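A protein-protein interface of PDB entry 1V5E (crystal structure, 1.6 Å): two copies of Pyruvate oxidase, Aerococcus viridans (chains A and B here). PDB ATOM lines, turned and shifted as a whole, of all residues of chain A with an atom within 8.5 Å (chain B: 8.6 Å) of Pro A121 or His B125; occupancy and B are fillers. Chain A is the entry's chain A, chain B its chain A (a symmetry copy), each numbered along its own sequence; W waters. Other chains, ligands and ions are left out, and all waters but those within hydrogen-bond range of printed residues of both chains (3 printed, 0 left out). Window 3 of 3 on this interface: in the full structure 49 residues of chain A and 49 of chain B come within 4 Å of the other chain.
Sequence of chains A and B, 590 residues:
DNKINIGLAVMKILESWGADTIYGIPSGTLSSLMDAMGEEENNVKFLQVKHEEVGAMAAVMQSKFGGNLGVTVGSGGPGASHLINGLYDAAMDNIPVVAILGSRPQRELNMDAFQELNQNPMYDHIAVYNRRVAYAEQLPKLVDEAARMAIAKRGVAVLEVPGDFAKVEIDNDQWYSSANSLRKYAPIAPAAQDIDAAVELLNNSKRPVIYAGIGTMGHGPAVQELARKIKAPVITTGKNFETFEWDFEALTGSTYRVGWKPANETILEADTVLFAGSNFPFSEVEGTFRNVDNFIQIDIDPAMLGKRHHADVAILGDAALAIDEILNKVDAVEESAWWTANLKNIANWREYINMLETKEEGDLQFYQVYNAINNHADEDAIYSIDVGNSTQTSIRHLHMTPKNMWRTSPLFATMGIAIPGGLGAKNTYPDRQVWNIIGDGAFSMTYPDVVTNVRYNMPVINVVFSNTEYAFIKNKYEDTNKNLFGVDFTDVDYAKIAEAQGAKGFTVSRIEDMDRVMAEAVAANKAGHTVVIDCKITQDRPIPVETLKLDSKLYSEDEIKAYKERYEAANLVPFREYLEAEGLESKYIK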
ATOM      1  N   ILE A  84     -17.834  24.822  14.257  1.00  0.00           N
ATOM      2  CA  ILE A  84     -17.881  24.206  12.936  1.00  0.00           C
ATOM      3  C   ILE A  84     -19.022  24.520  11.970  1.00  0.00           C
ATOM      4  O   ILE A  84     -18.756  24.891  10.827  1.00  0.00           O
ATOM      5  CB  ILE A  84     -17.688  22.666  13.029  1.00  0.00           C
ATOM      6  CG1 ILE A  84     -17.341  22.115  11.644  1.00  0.00           C
ATOM      7  CG2 ILE A  84     -18.949  21.993  13.567  1.00  0.00           C
ATOM      8  CD1 ILE A  84     -16.688  20.746  11.681  1.00  0.00           C
ATOM      9  N   TYR A  88     -18.337  26.468   8.459  1.00  0.00           N
ATOM     10  CA  TYR A  88     -18.560  25.809   7.180  1.00  0.00           C
ATOM     11  C   TYR A  88     -19.522  26.661   6.353  1.00  0.00           C
ATOM     12  O   TYR A  88     -19.352  26.812   5.143  1.00  0.00           O
ATOM     13  CB  TYR A  88     -19.118  24.397   7.393  1.00  0.00           C
ATOM     14  CG  TYR A  88     -18.060  23.320   7.250  1.00  0.00           C
ATOM     15  CD1 TYR A  88     -17.915  22.613   6.055  1.00  0.00           C
ATOM     16  CD2 TYR A  88     -17.174  23.046   8.289  1.00  0.00           C
ATOM     17  CE1 TYR A  88     -16.907  21.658   5.896  1.00  0.00           C
ATOM     18  CE2 TYR A  88     -16.159  22.093   8.143  1.00  0.00           C
ATOM     19  CZ  TYR A  88     -16.035  21.408   6.942  1.00  0.00           C
ATOM     20  OH  TYR A  88     -15.024  20.485   6.784  1.00  0.00           O
ATOM     21  N   LEU A 101      -9.542  30.412  18.245  1.00  0.00           N
ATOM     22  CA  LEU A 101      -9.627  29.191  19.028  1.00  0.00           C
ATOM     23  C   LEU A 101      -8.732  29.326  20.250  1.00  0.00           C
ATOM     24  O   LEU A 101      -7.520  29.504  20.124  1.00  0.00           O
ATOM     25  CB  LEU A 101      -9.167  27.991  18.196  1.00  0.00           C
ATOM     26  CG  LEU A 101     -10.134  27.278  17.250  1.00  0.00           C
ATOM     27  CD1 LEU A 101     -11.131  28.240  16.636  1.00  0.00           C
ATOM     28  CD2 LEU A 101      -9.311  26.563  16.184  1.00  0.00           C
ATOM     29  N   LEU A 117      -4.810  19.887  22.924  1.00  0.00           N
ATOM     30  CA  LEU A 117      -4.725  19.140  21.676  1.00  0.00           C
ATOM     31  C   LEU A 117      -4.326  20.017  20.504  1.00  0.00           C
ATOM     32  O   LEU A 117      -4.416  21.240  20.563  1.00  0.00           O
ATOM     33  CB  LEU A 117      -6.080  18.496  21.351  1.00  0.00           C
ATOM     34  CG  LEU A 117      -7.194  19.400  20.802  1.00  0.00           C
ATOM     35  CD1 LEU A 117      -8.387  18.542  20.400  1.00  0.00           C
ATOM     36  CD2 LEU A 117      -7.607  20.440  21.839  1.00  0.00           C
ATOM     37  N   ASN A 118      -3.888  19.373  19.431  1.00  0.00           N
ATOM     38  CA  ASN A 118      -3.516  20.092  18.226  1.00  0.00           C
ATOM     39  C   ASN A 118      -4.809  20.451  17.497  1.00  0.00           C
ATOM     40  O   ASN A 118      -5.505  19.575  16.988  1.00  0.00           O
ATOM     41  CB  ASN A 118      -2.630  19.205  17.348  1.00  0.00           C
ATOM     42  CG  ASN A 118      -2.341  19.819  15.998  1.00  0.00           C
ATOM     43  OD1 ASN A 118      -2.491  21.028  15.805  1.00  0.00           O
ATOM     44  ND2 ASN A 118      -1.910  18.990  15.057  1.00  0.00           N
ATOM     45  N   GLN A 119      -5.135  21.738  17.457  1.00  0.00           N
ATOM     46  CA  GLN A 119      -6.358  22.178  16.798  1.00  0.00           C
ATOM     47  C   GLN A 119      -6.127  22.699  15.384  1.00  0.00           C
ATOM     48  O   GLN A 119      -7.045  23.212  14.749  1.00  0.00           O
ATOM     49  CB  GLN A 119      -7.041  23.261  17.638  1.00  0.00           C
ATOM     50  CG  GLN A 119      -7.318  22.823  19.068  1.00  0.00           C
ATOM     51  CD  GLN A 119      -7.977  23.904  19.893  1.00  0.00           C
ATOM     52  OE1 GLN A 119      -9.202  23.943  20.034  1.00  0.00           O
ATOM     53  NE2 GLN A 119      -7.166  24.797  20.440  1.00  0.00           N
ATOM     54  N   ASN A 120      -4.909  22.558  14.875  1.00  0.00           N
ATOM     55  CA  ASN A 120      -4.640  23.051  13.532  1.00  0.00           C
ATOM     56  C   ASN A 120      -5.393  22.275  12.446  1.00  0.00           C
ATOM     57  O   ASN A 120      -5.830  22.857  11.458  1.00  0.00           O
ATOM     58  CB  ASN A 120      -3.137  23.035  13.248  1.00  0.00           C
ATOM     59  CG  ASN A 120      -2.777  23.807  11.993  1.00  0.00           C
ATOM     60  OD1 ASN A 120      -2.479  23.221  10.955  1.00  0.00           O
ATOM     61  ND2 ASN A 120      -2.814  25.133  12.082  1.00  0.00           N
ATOM     62  N   PRO A 121      -5.550  20.951  12.610  1.00  0.00           N
ATOM     63  CA  PRO A 121      -6.269  20.178  11.589  1.00  0.00           C
ATOM     64  C   PRO A 121      -7.763  20.487  11.510  1.00  0.00           C
ATOM     65  O   PRO A 121      -8.376  20.371  10.452  1.00  0.00           O
ATOM     66  CB  PRO A 121      -6.027  18.729  12.017  1.00  0.00           C
ATOM     67  CG  PRO A 121      -4.700  18.788  12.681  1.00  0.00           C
ATOM     68  CD  PRO A 121      -4.809  20.050  13.512  1.00  0.00           C
ATOM     69  N   MET A 122      -8.335  20.894  12.638  1.00  0.00           N
ATOM     70  CA  MET A 122      -9.767  21.168  12.736  1.00  0.00           C
ATOM     71  C   MET A 122     -10.423  21.916  11.576  1.00  0.00           C
ATOM     72  O   MET A 122     -11.410  21.439  11.004  1.00  0.00           O
ATOM     73  CB  MET A 122     -10.063  21.899  14.052  1.00  0.00           C
ATOM     74  CG  MET A 122     -11.524  21.818  14.482  1.00  0.00           C
ATOM     75  SD  MET A 122     -11.807  22.530  16.124  1.00  0.00           S
ATOM     76  CE  MET A 122     -11.133  21.260  17.181  1.00  0.00           C
ATOM     77  N   TYR A 123      -9.879  23.072  11.212  1.00  0.00           N
ATOM     78  CA  TYR A 123     -10.472  23.879  10.147  1.00  0.00           C
ATOM     79  C   TYR A 123      -9.570  24.152   8.951  1.00  0.00           C
ATOM     80  O   TYR A 123      -9.873  25.004   8.118  1.00  0.00           O
ATOM     81  CB  TYR A 123     -10.962  25.209  10.736  1.00  0.00           C
ATOM     82  CG  TYR A 123     -12.036  25.020  11.784  1.00  0.00           C
ATOM     83  CD1 TYR A 123     -13.222  24.366  11.467  1.00  0.00           C
ATOM     84  CD2 TYR A 123     -11.848  25.449  13.101  1.00  0.00           C
ATOM     85  CE1 TYR A 123     -14.198  24.128  12.430  1.00  0.00           C
ATOM     86  CE2 TYR A 123     -12.828  25.217  14.081  1.00  0.00           C
ATOM     87  CZ  TYR A 123     -13.996  24.551  13.731  1.00  0.00           C
ATOM     88  OH  TYR A 123     -14.962  24.280  14.676  1.00  0.00           O
ATOM     89  N   ASP A 124      -8.476  23.411   8.842  1.00  0.00           N
ATOM     90  CA  ASP A 124      -7.560  23.644   7.737  1.00  0.00           C
ATOM     91  C   ASP A 124      -8.206  23.509   6.359  1.00  0.00           C
ATOM     92  O   ASP A 124      -7.877  24.253   5.437  1.00  0.00           O
ATOM     93  CB  ASP A 124      -6.368  22.696   7.823  1.00  0.00           C
ATOM     94  CG  ASP A 124      -5.238  23.127   6.922  1.00  0.00           C
ATOM     95  OD1 ASP A 124      -4.727  24.246   7.127  1.00  0.00           O
ATOM     96  OD2 ASP A 124      -4.874  22.355   6.010  1.00  0.00           O
ATOM     97  N   HIS A 125      -9.132  22.570   6.222  1.00  0.00           N
ATOM     98  CA  HIS A 125      -9.790  22.341   4.939  1.00  0.00           C
ATOM     99  C   HIS A 125     -10.639  23.505   4.428  1.00  0.00           C
ATOM    100  O   HIS A 125     -10.678  23.770   3.225  1.00  0.00           O
ATOM    101  CB  HIS A 125     -10.665  21.089   5.020  1.00  0.00           C
ATOM    102  CG  HIS A 125     -11.418  20.804   3.760  1.00  0.00           C
ATOM    103  ND1 HIS A 125     -10.793  20.431   2.589  1.00  0.00           N
ATOM    104  CD2 HIS A 125     -12.740  20.874   3.477  1.00  0.00           C
ATOM    105  CE1 HIS A 125     -11.699  20.286   1.638  1.00  0.00           C
ATOM    106  NE2 HIS A 125     -12.887  20.550   2.150  1.00  0.00           N
ATOM    107  N   ILE A 126     -11.306  24.208   5.338  1.00  0.00           N
ATOM    108  CA  ILE A 126     -12.187  25.304   4.945  1.00  0.00           C
ATOM    109  C   ILE A 126     -11.654  26.717   5.134  1.00  0.00           C
ATOM    110  O   ILE A 126     -12.237  27.670   4.613  1.00  0.00           O
ATOM    111  CB  ILE A 126     -13.525  25.229   5.707  1.00  0.00           C
ATOM    112  CG1 ILE A 126     -13.285  25.465   7.201  1.00  0.00           C
ATOM    113  CG2 ILE A 126     -14.176  23.872   5.489  1.00  0.00           C
ATOM    114  CD1 ILE A 126     -14.552  25.661   8.004  1.00  0.00           C
ATOM    115  N   ALA A 127     -10.554  26.862   5.863  1.00  0.00           N
ATOM    116  CA  ALA A 127     -10.006  28.188   6.148  1.00  0.00           C
ATOM    117  C   ALA A 127      -9.143  28.826   5.067  1.00  0.00           C
ATOM    118  O   ALA A 127      -8.476  28.133   4.302  1.00  0.00           O
ATOM    119  CB  ALA A 127      -9.225  28.140   7.451  1.00  0.00           C
ATOM    120  N   ASN A 130      -5.079  29.765   8.580  1.00  0.00           N
ATOM    121  CA  ASN A 130      -5.219  28.850   9.715  1.00  0.00           C
ATOM    122  C   ASN A 130      -3.877  28.609  10.394  1.00  0.00           C
ATOM    123  O   ASN A 130      -3.109  27.735   9.989  1.00  0.00           O
ATOM    124  CB  ASN A 130      -5.818  27.536   9.203  1.00  0.00           C
ATOM    125  CG  ASN A 130      -5.950  26.494  10.282  1.00  0.00           C
ATOM    126  OD1 ASN A 130      -6.448  26.776  11.369  1.00  0.00           O
ATOM    127  ND2 ASN A 130      -5.515  25.276   9.984  1.00  0.00           N
ATOM    128  N   ARG A 132      -1.406  28.540  14.230  1.00  0.00           N
ATOM    129  CA  ARG A 132      -1.296  28.448  15.676  1.00  0.00           C
ATOM    130  C   ARG A 132      -0.211  29.450  16.052  1.00  0.00           C
ATOM    131  O   ARG A 132       0.941  29.298  15.649  1.00  0.00           O
ATOM    132  CB  ARG A 132      -0.873  27.043  16.122  1.00  0.00           C
ATOM    133  CG  ARG A 132      -0.424  26.995  17.579  1.00  0.00           C
ATOM    134  CD  ARG A 132      -0.002  25.600  18.029  1.00  0.00           C
ATOM    135  NE  ARG A 132      -1.146  24.780  18.414  1.00  0.00           N
ATOM    136  CZ  ARG A 132      -1.058  23.650  19.110  1.00  0.00           C
ATOM    137  NH1 ARG A 132       0.126  23.192  19.495  1.00  0.00           N
ATOM    138  NH2 ARG A 132      -2.161  22.998  19.457  1.00  0.00           N
ATOM    139  N   GLU A 160      -5.234  29.936  16.410  1.00  0.00           N
ATOM    140  CA  GLU A 160      -5.257  29.166  17.651  1.00  0.00           C
ATOM    141  C   GLU A 160      -4.342  29.954  18.579  1.00  0.00           C
ATOM    142  O   GLU A 160      -3.157  30.142  18.287  1.00  0.00           O
ATOM    143  CB  GLU A 160      -4.725  27.751  17.435  1.00  0.00           C
ATOM    144  CG  GLU A 160      -4.820  26.894  18.691  1.00  0.00           C
ATOM    145  CD  GLU A 160      -4.307  25.485  18.487  1.00  0.00           C
ATOM    146  OE1 GLU A 160      -3.735  25.210  17.410  1.00  0.00           O
ATOM    147  OE2 GLU A 160      -4.470  24.658  19.407  1.00  0.00           O
ATOM    148  N   ILE B  84     -19.136  16.432  15.633  1.00  0.00           N
ATOM    149  CA  ILE B  84     -17.782  16.705  16.099  1.00  0.00           C
ATOM    150  C   ILE B  84     -17.432  16.599  17.583  1.00  0.00           C
ATOM    151  O   ILE B  84     -16.474  15.907  17.926  1.00  0.00           O
ATOM    152  CB  ILE B  84     -17.258  18.057  15.538  1.00  0.00           C
ATOM    153  CG1 ILE B  84     -15.738  18.119  15.702  1.00  0.00           C
ATOM    154  CG2 ILE B  84     -17.917  19.234  16.255  1.00  0.00           C
ATOM    155  CD1 ILE B  84     -15.069  19.141  14.803  1.00  0.00           C
ATOM    156  N   TYR B  88     -14.817  13.786  18.937  1.00  0.00           N
ATOM    157  CA  TYR B  88     -13.544  14.169  19.530  1.00  0.00           C
ATOM    158  C   TYR B  88     -13.444  13.543  20.920  1.00  0.00           C
ATOM    159  O   TYR B  88     -12.383  13.069  21.326  1.00  0.00           O
ATOM    160  CB  TYR B  88     -13.423  15.695  19.602  1.00  0.00           C
ATOM    161  CG  TYR B  88     -12.563  16.269  18.492  1.00  0.00           C
ATOM    162  CD1 TYR B  88     -11.222  16.587  18.717  1.00  0.00           C
ATOM    163  CD2 TYR B  88     -13.076  16.446  17.209  1.00  0.00           C
ATOM    164  CE1 TYR B  88     -10.409  17.064  17.685  1.00  0.00           C
ATOM    165  CE2 TYR B  88     -12.272  16.921  16.167  1.00  0.00           C
ATOM    166  CZ  TYR B  88     -10.941  17.225  16.417  1.00  0.00           C
ATOM    167  OH  TYR B  88     -10.138  17.672  15.390  1.00  0.00           O
ATOM    168  N   ALA B  91     -12.628   9.919  20.483  1.00  0.00           N
ATOM    169  CA  ALA B  91     -11.255   9.781  20.015  1.00  0.00           C
ATOM    170  C   ALA B  91     -10.249   9.916  21.151  1.00  0.00           C
ATOM    171  O   ALA B  91      -9.331   9.107  21.278  1.00  0.00           O
ATOM    172  CB  ALA B  91     -10.966  10.819  18.937  1.00  0.00           C
ATOM    173  N   MET B  92     -10.422  10.938  21.977  1.00  0.00           N
ATOM    174  CA  MET B  92      -9.506  11.161  23.081  1.00  0.00           C
ATOM    175  C   MET B  92      -9.659  10.140  24.207  1.00  0.00           C
ATOM    176  O   MET B  92      -8.693   9.843  24.910  1.00  0.00           O
ATOM    177  CB  MET B  92      -9.664  12.591  23.604  1.00  0.00           C
ATOM    178  CG  MET B  92      -9.283  13.637  22.559  1.00  0.00           C
ATOM    179  SD  MET B  92      -9.010  15.291  23.222  1.00  0.00           S
ATOM    180  CE  MET B  92      -7.370  15.114  23.927  1.00  0.00           C
ATOM    181  N   ASN B 120     -14.525  14.097   3.556  1.00  0.00           N
ATOM    182  CA  ASN B 120     -13.433  13.247   4.010  1.00  0.00           C
ATOM    183  C   ASN B 120     -12.466  13.967   4.955  1.00  0.00           C
ATOM    184  O   ASN B 120     -11.954  13.364   5.895  1.00  0.00           O
ATOM    185  CB  ASN B 120     -12.673  12.669   2.815  1.00  0.00           C
ATOM    186  CG  ASN B 120     -11.726  11.554   3.216  1.00  0.00           C
ATOM    187  OD1 ASN B 120     -10.513  11.744   3.267  1.00  0.00           O
ATOM    188  ND2 ASN B 120     -12.282  10.383   3.514  1.00  0.00           N
ATOM    189  N   PRO B 121     -12.198  15.262   4.719  1.00  0.00           N
ATOM    190  CA  PRO B 121     -11.277  15.982   5.609  1.00  0.00           C
ATOM    191  C   PRO B 121     -11.821  16.207   7.019  1.00  0.00           C
ATOM    192  O   PRO B 121     -11.062  16.285   7.982  1.00  0.00           O
ATOM    193  CB  PRO B 121     -11.062  17.310   4.882  1.00  0.00           C
ATOM    194  CG  PRO B 121     -11.215  16.944   3.451  1.00  0.00           C
ATOM    195  CD  PRO B 121     -12.420  16.026   3.478  1.00  0.00           C
ATOM    196  N   MET B 122     -13.141  16.296   7.128  1.00  0.00           N
ATOM    197  CA  MET B 122     -13.806  16.572   8.400  1.00  0.00           C
ATOM    198  C   MET B 122     -13.276  15.857   9.642  1.00  0.00           C
ATOM    199  O   MET B 122     -12.942  16.506  10.641  1.00  0.00           O
ATOM    200  CB  MET B 122     -15.312  16.314   8.261  1.00  0.00           C
ATOM    201  CG  MET B 122     -16.152  16.998   9.334  1.00  0.00           C
ATOM    202  SD  MET B 122     -17.931  16.828   9.040  1.00  0.00           S
ATOM    203  CE  MET B 122     -18.183  17.987   7.707  1.00  0.00           C
ATOM    204  N   TYR B 123     -13.180  14.533   9.588  1.00  0.00           N
ATOM    205  CA  TYR B 123     -12.732  13.764  10.748  1.00  0.00           C
ATOM    206  C   TYR B 123     -11.479  12.927  10.535  1.00  0.00           C
ATOM    207  O   TYR B 123     -11.152  12.068  11.353  1.00  0.00           O
ATOM    208  CB  TYR B 123     -13.878  12.863  11.228  1.00  0.00           C
ATOM    209  CG  TYR B 123     -15.090  13.652  11.673  1.00  0.00           C
ATOM    210  CD1 TYR B 123     -14.984  14.589  12.696  1.00  0.00           C
ATOM    211  CD2 TYR B 123     -16.328  13.499  11.043  1.00  0.00           C
ATOM    212  CE1 TYR B 123     -16.071  15.368  13.081  1.00  0.00           C
ATOM    213  CE2 TYR B 123     -17.433  14.278  11.425  1.00  0.00           C
ATOM    214  CZ  TYR B 123     -17.287  15.211  12.443  1.00  0.00           C
ATOM    215  OH  TYR B 123     -18.344  16.013  12.819  1.00  0.00           O
ATOM    216  N   ASP B 124     -10.755  13.190   9.456  1.00  0.00           N
ATOM    217  CA  ASP B 124      -9.563  12.404   9.184  1.00  0.00           C
ATOM    218  C   ASP B 124      -8.530  12.438  10.308  1.00  0.00           C
ATOM    219  O   ASP B 124      -7.874  11.435  10.587  1.00  0.00           O
ATOM    220  CB  ASP B 124      -8.904  12.867   7.888  1.00  0.00           C
ATOM    221  CG  ASP B 124      -7.886  11.873   7.386  1.00  0.00           C
ATOM    222  OD1 ASP B 124      -8.286  10.724   7.108  1.00  0.00           O
ATOM    223  OD2 ASP B 124      -6.697  12.237   7.283  1.00  0.00           O
ATOM    224  N   HIS B 125      -8.392  13.584  10.961  1.00  0.00           N
ATOM    225  CA  HIS B 125      -7.413  13.728  12.034  1.00  0.00           C
ATOM    226  C   HIS B 125      -7.661  12.853  13.262  1.00  0.00           C
ATOM    227  O   HIS B 125      -6.716  12.349  13.874  1.00  0.00           O
ATOM    228  CB  HIS B 125      -7.340  15.190  12.477  1.00  0.00           C
ATOM    229  CG  HIS B 125      -6.392  15.425  13.610  1.00  0.00           C
ATOM    230  ND1 HIS B 125      -5.028  15.276  13.482  1.00  0.00           N
ATOM    231  CD2 HIS B 125      -6.615  15.760  14.903  1.00  0.00           C
ATOM    232  CE1 HIS B 125      -4.451  15.507  14.648  1.00  0.00           C
ATOM    233  NE2 HIS B 125      -5.392  15.801  15.527  1.00  0.00           N
ATOM    234  N   ILE B 126      -8.927  12.657  13.616  1.00  0.00           N
ATOM    235  CA  ILE B 126      -9.265  11.880  14.805  1.00  0.00           C
ATOM    236  C   ILE B 126      -9.747  10.453  14.583  1.00  0.00           C
ATOM    237  O   ILE B 126      -9.822   9.673  15.533  1.00  0.00           O
ATOM    238  CB  ILE B 126     -10.356  12.592  15.630  1.00  0.00           C
ATOM    239  CG1 ILE B 126     -11.663  12.636  14.833  1.00  0.00           C
ATOM    240  CG2 ILE B 126      -9.909  14.003  15.981  1.00  0.00           C
ATOM    241  CD1 ILE B 126     -12.861  13.087  15.640  1.00  0.00           C
ATOM    242  N   ALA B 127     -10.064  10.103  13.341  1.00  0.00           N
ATOM    243  CA  ALA B 127     -10.593   8.772  13.044  1.00  0.00           C
ATOM    244  C   ALA B 127      -9.581   7.642  12.900  1.00  0.00           C
ATOM    245  O   ALA B 127      -8.445   7.862  12.487  1.00  0.00           O
ATOM    246  CB  ALA B 127     -11.451   8.841  11.792  1.00  0.00           C
ATOM    247  N   VAL B 128     -10.014   6.431  13.251  1.00  0.00           N
ATOM    248  CA  VAL B 128      -9.177   5.240  13.115  1.00  0.00           C
ATOM    249  C   VAL B 128      -9.499   4.602  11.767  1.00  0.00           C
ATOM    250  O   VAL B 128      -8.782   3.715  11.298  1.00  0.00           O
ATOM    251  CB  VAL B 128      -9.452   4.198  14.232  1.00  0.00           C
ATOM    252  CG1 VAL B 128      -9.105   4.789  15.587  1.00  0.00           C
ATOM    253  CG2 VAL B 128     -10.908   3.749  14.199  1.00  0.00           C
ATOM    254  N   TYR B 129     -10.579   5.077  11.152  1.00  0.00           N
ATOM    255  CA  TYR B 129     -11.060   4.596   9.856  1.00  0.00           C
ATOM    256  C   TYR B 129     -11.877   5.766   9.294  1.00  0.00           C
ATOM    257  O   TYR B 129     -12.741   6.303   9.984  1.00  0.00           O
ATOM    258  CB  TYR B 129     -11.956   3.372  10.069  1.00  0.00           C
ATOM    259  CG  TYR B 129     -12.236   2.531   8.840  1.00  0.00           C
ATOM    260  CD1 TYR B 129     -11.262   1.682   8.315  1.00  0.00           C
ATOM    261  CD2 TYR B 129     -13.496   2.533   8.244  1.00  0.00           C
ATOM    262  CE1 TYR B 129     -11.539   0.845   7.233  1.00  0.00           C
ATOM    263  CE2 TYR B 129     -13.784   1.706   7.162  1.00  0.00           C
ATOM    264  CZ  TYR B 129     -12.801   0.860   6.664  1.00  0.00           C
ATOM    265  OH  TYR B 129     -13.091   0.017   5.612  1.00  0.00           O
ATOM    266  N   ASN B 130     -11.609   6.170   8.057  1.00  0.00           N
ATOM    267  CA  ASN B 130     -12.327   7.309   7.483  1.00  0.00           C
ATOM    268  C   ASN B 130     -12.384   7.214   5.963  1.00  0.00           C
ATOM    269  O   ASN B 130     -11.464   7.645   5.266  1.00  0.00           O
ATOM    270  CB  ASN B 130     -11.621   8.595   7.925  1.00  0.00           C
ATOM    271  CG  ASN B 130     -12.244   9.835   7.339  1.00  0.00           C
ATOM    272  OD1 ASN B 130     -13.460  10.003   7.371  1.00  0.00           O
ATOM    273  ND2 ASN B 130     -11.409  10.720   6.807  1.00  0.00           N
ATOM    274  N   VAL B 156     -12.951   6.098  16.694  1.00  0.00           N
ATOM    275  CA  VAL B 156     -13.984   6.529  15.765  1.00  0.00           C
ATOM    276  C   VAL B 156     -13.799   6.040  14.331  1.00  0.00           C
ATOM    277  O   VAL B 156     -12.812   6.376  13.681  1.00  0.00           O
ATOM    278  CB  VAL B 156     -14.053   8.071  15.737  1.00  0.00           C
ATOM    279  CG1 VAL B 156     -15.160   8.539  14.806  1.00  0.00           C
ATOM    280  CG2 VAL B 156     -14.267   8.608  17.147  1.00  0.00           C
ATOM    281  N   VAL B 158     -15.353   6.256  10.661  1.00  0.00           N
ATOM    282  CA  VAL B 158     -16.256   7.113   9.894  1.00  0.00           C
ATOM    283  C   VAL B 158     -16.460   6.684   8.444  1.00  0.00           C
ATOM    284  O   VAL B 158     -15.500   6.384   7.731  1.00  0.00           O
ATOM    285  CB  VAL B 158     -15.738   8.574   9.912  1.00  0.00           C
ATOM    286  CG1 VAL B 158     -16.737   9.512   9.245  1.00  0.00           C
ATOM    287  CG2 VAL B 158     -15.474   9.006  11.342  1.00  0.00           C
HETATM  288  O   HOH W   1      -7.862  19.439  15.297  1.00  0.00           O
HETATM  289  O   HOH W   2     -14.795  18.061   5.240  1.00  0.00           O
HETATM  290  O   HOH W   3      -5.925  16.852  18.092  1.00  0.00           O
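Hydrophobic or aromatic side chains of chain B within 4 Å of the printed part of chain A: Ile B84, Tyr B88, Pro B121 and His B125.
Printed residues of chain B within 4 Å of Ile A84: Ile B84. Asn A120 touches none of the printed residues of chain B. Pro A121 touches just one residue of chain B: His B125 (3.6 Å). Printed residues of chain A within 4 Å of Ile B84: Ile A84 (3.9 Å). Of the printed residues of chain A, Tyr B88 touches Leu A117 (3.7 Å). Of chain A, only Pro A121 (3.6 Å) comes within 4 Å of His B125.
N of Ile A84 is in hydrogen-bond range of OH of Tyr A123 (3.0 Å). The guanidinium group (NH2) of Arg A132 is in hydrogen-bond range of the backbone carbonyl oxygen (O) of Leu A117. N of Ile B84 is in hydrogen-bond range of OH of Tyr B123 (3.0 Å).
CD1 of Ile B84 touches CD1 of Ile A84 (3.9 Å). Leu A117 touches Tyr B88. ND1 of His B125 touches CG of Pro A121, 3.6 Å away. Pro B121 touches His A125 (CG to ND1, 3.6 Å).
Water W3 bridges NE2 of His B125 (2.8 Å) and O of Asn A118 (3.0 Å). Water W2 lies within hydrogen-bond range of the side-chain hydroxyl (OH) of Tyr A88 (2.9 Å) and the backbone NH (N) of Met B122 (3.1 Å). Water W1 lies within hydrogen-bond range of the side-chain hydroxyl of Tyr B88 (2.9 Å), the backbone carbonyl oxygen of Asn A118 (2.9 Å) and the backbone NH of Met A122 (3.1 Å).
Ile B84 touches its own counterpart, Ile A84. Pro A121 touches His B125, and with the chains exchanged His A125 touches Pro B121. Positions printed for both chains: 84, 88, 120, 121, 122, 123, 124, 125, 126, 127 and 130. Of the 4 pairs that touch across the chains among the printed residues, 3 have their exchanged pair printed and touching as well.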
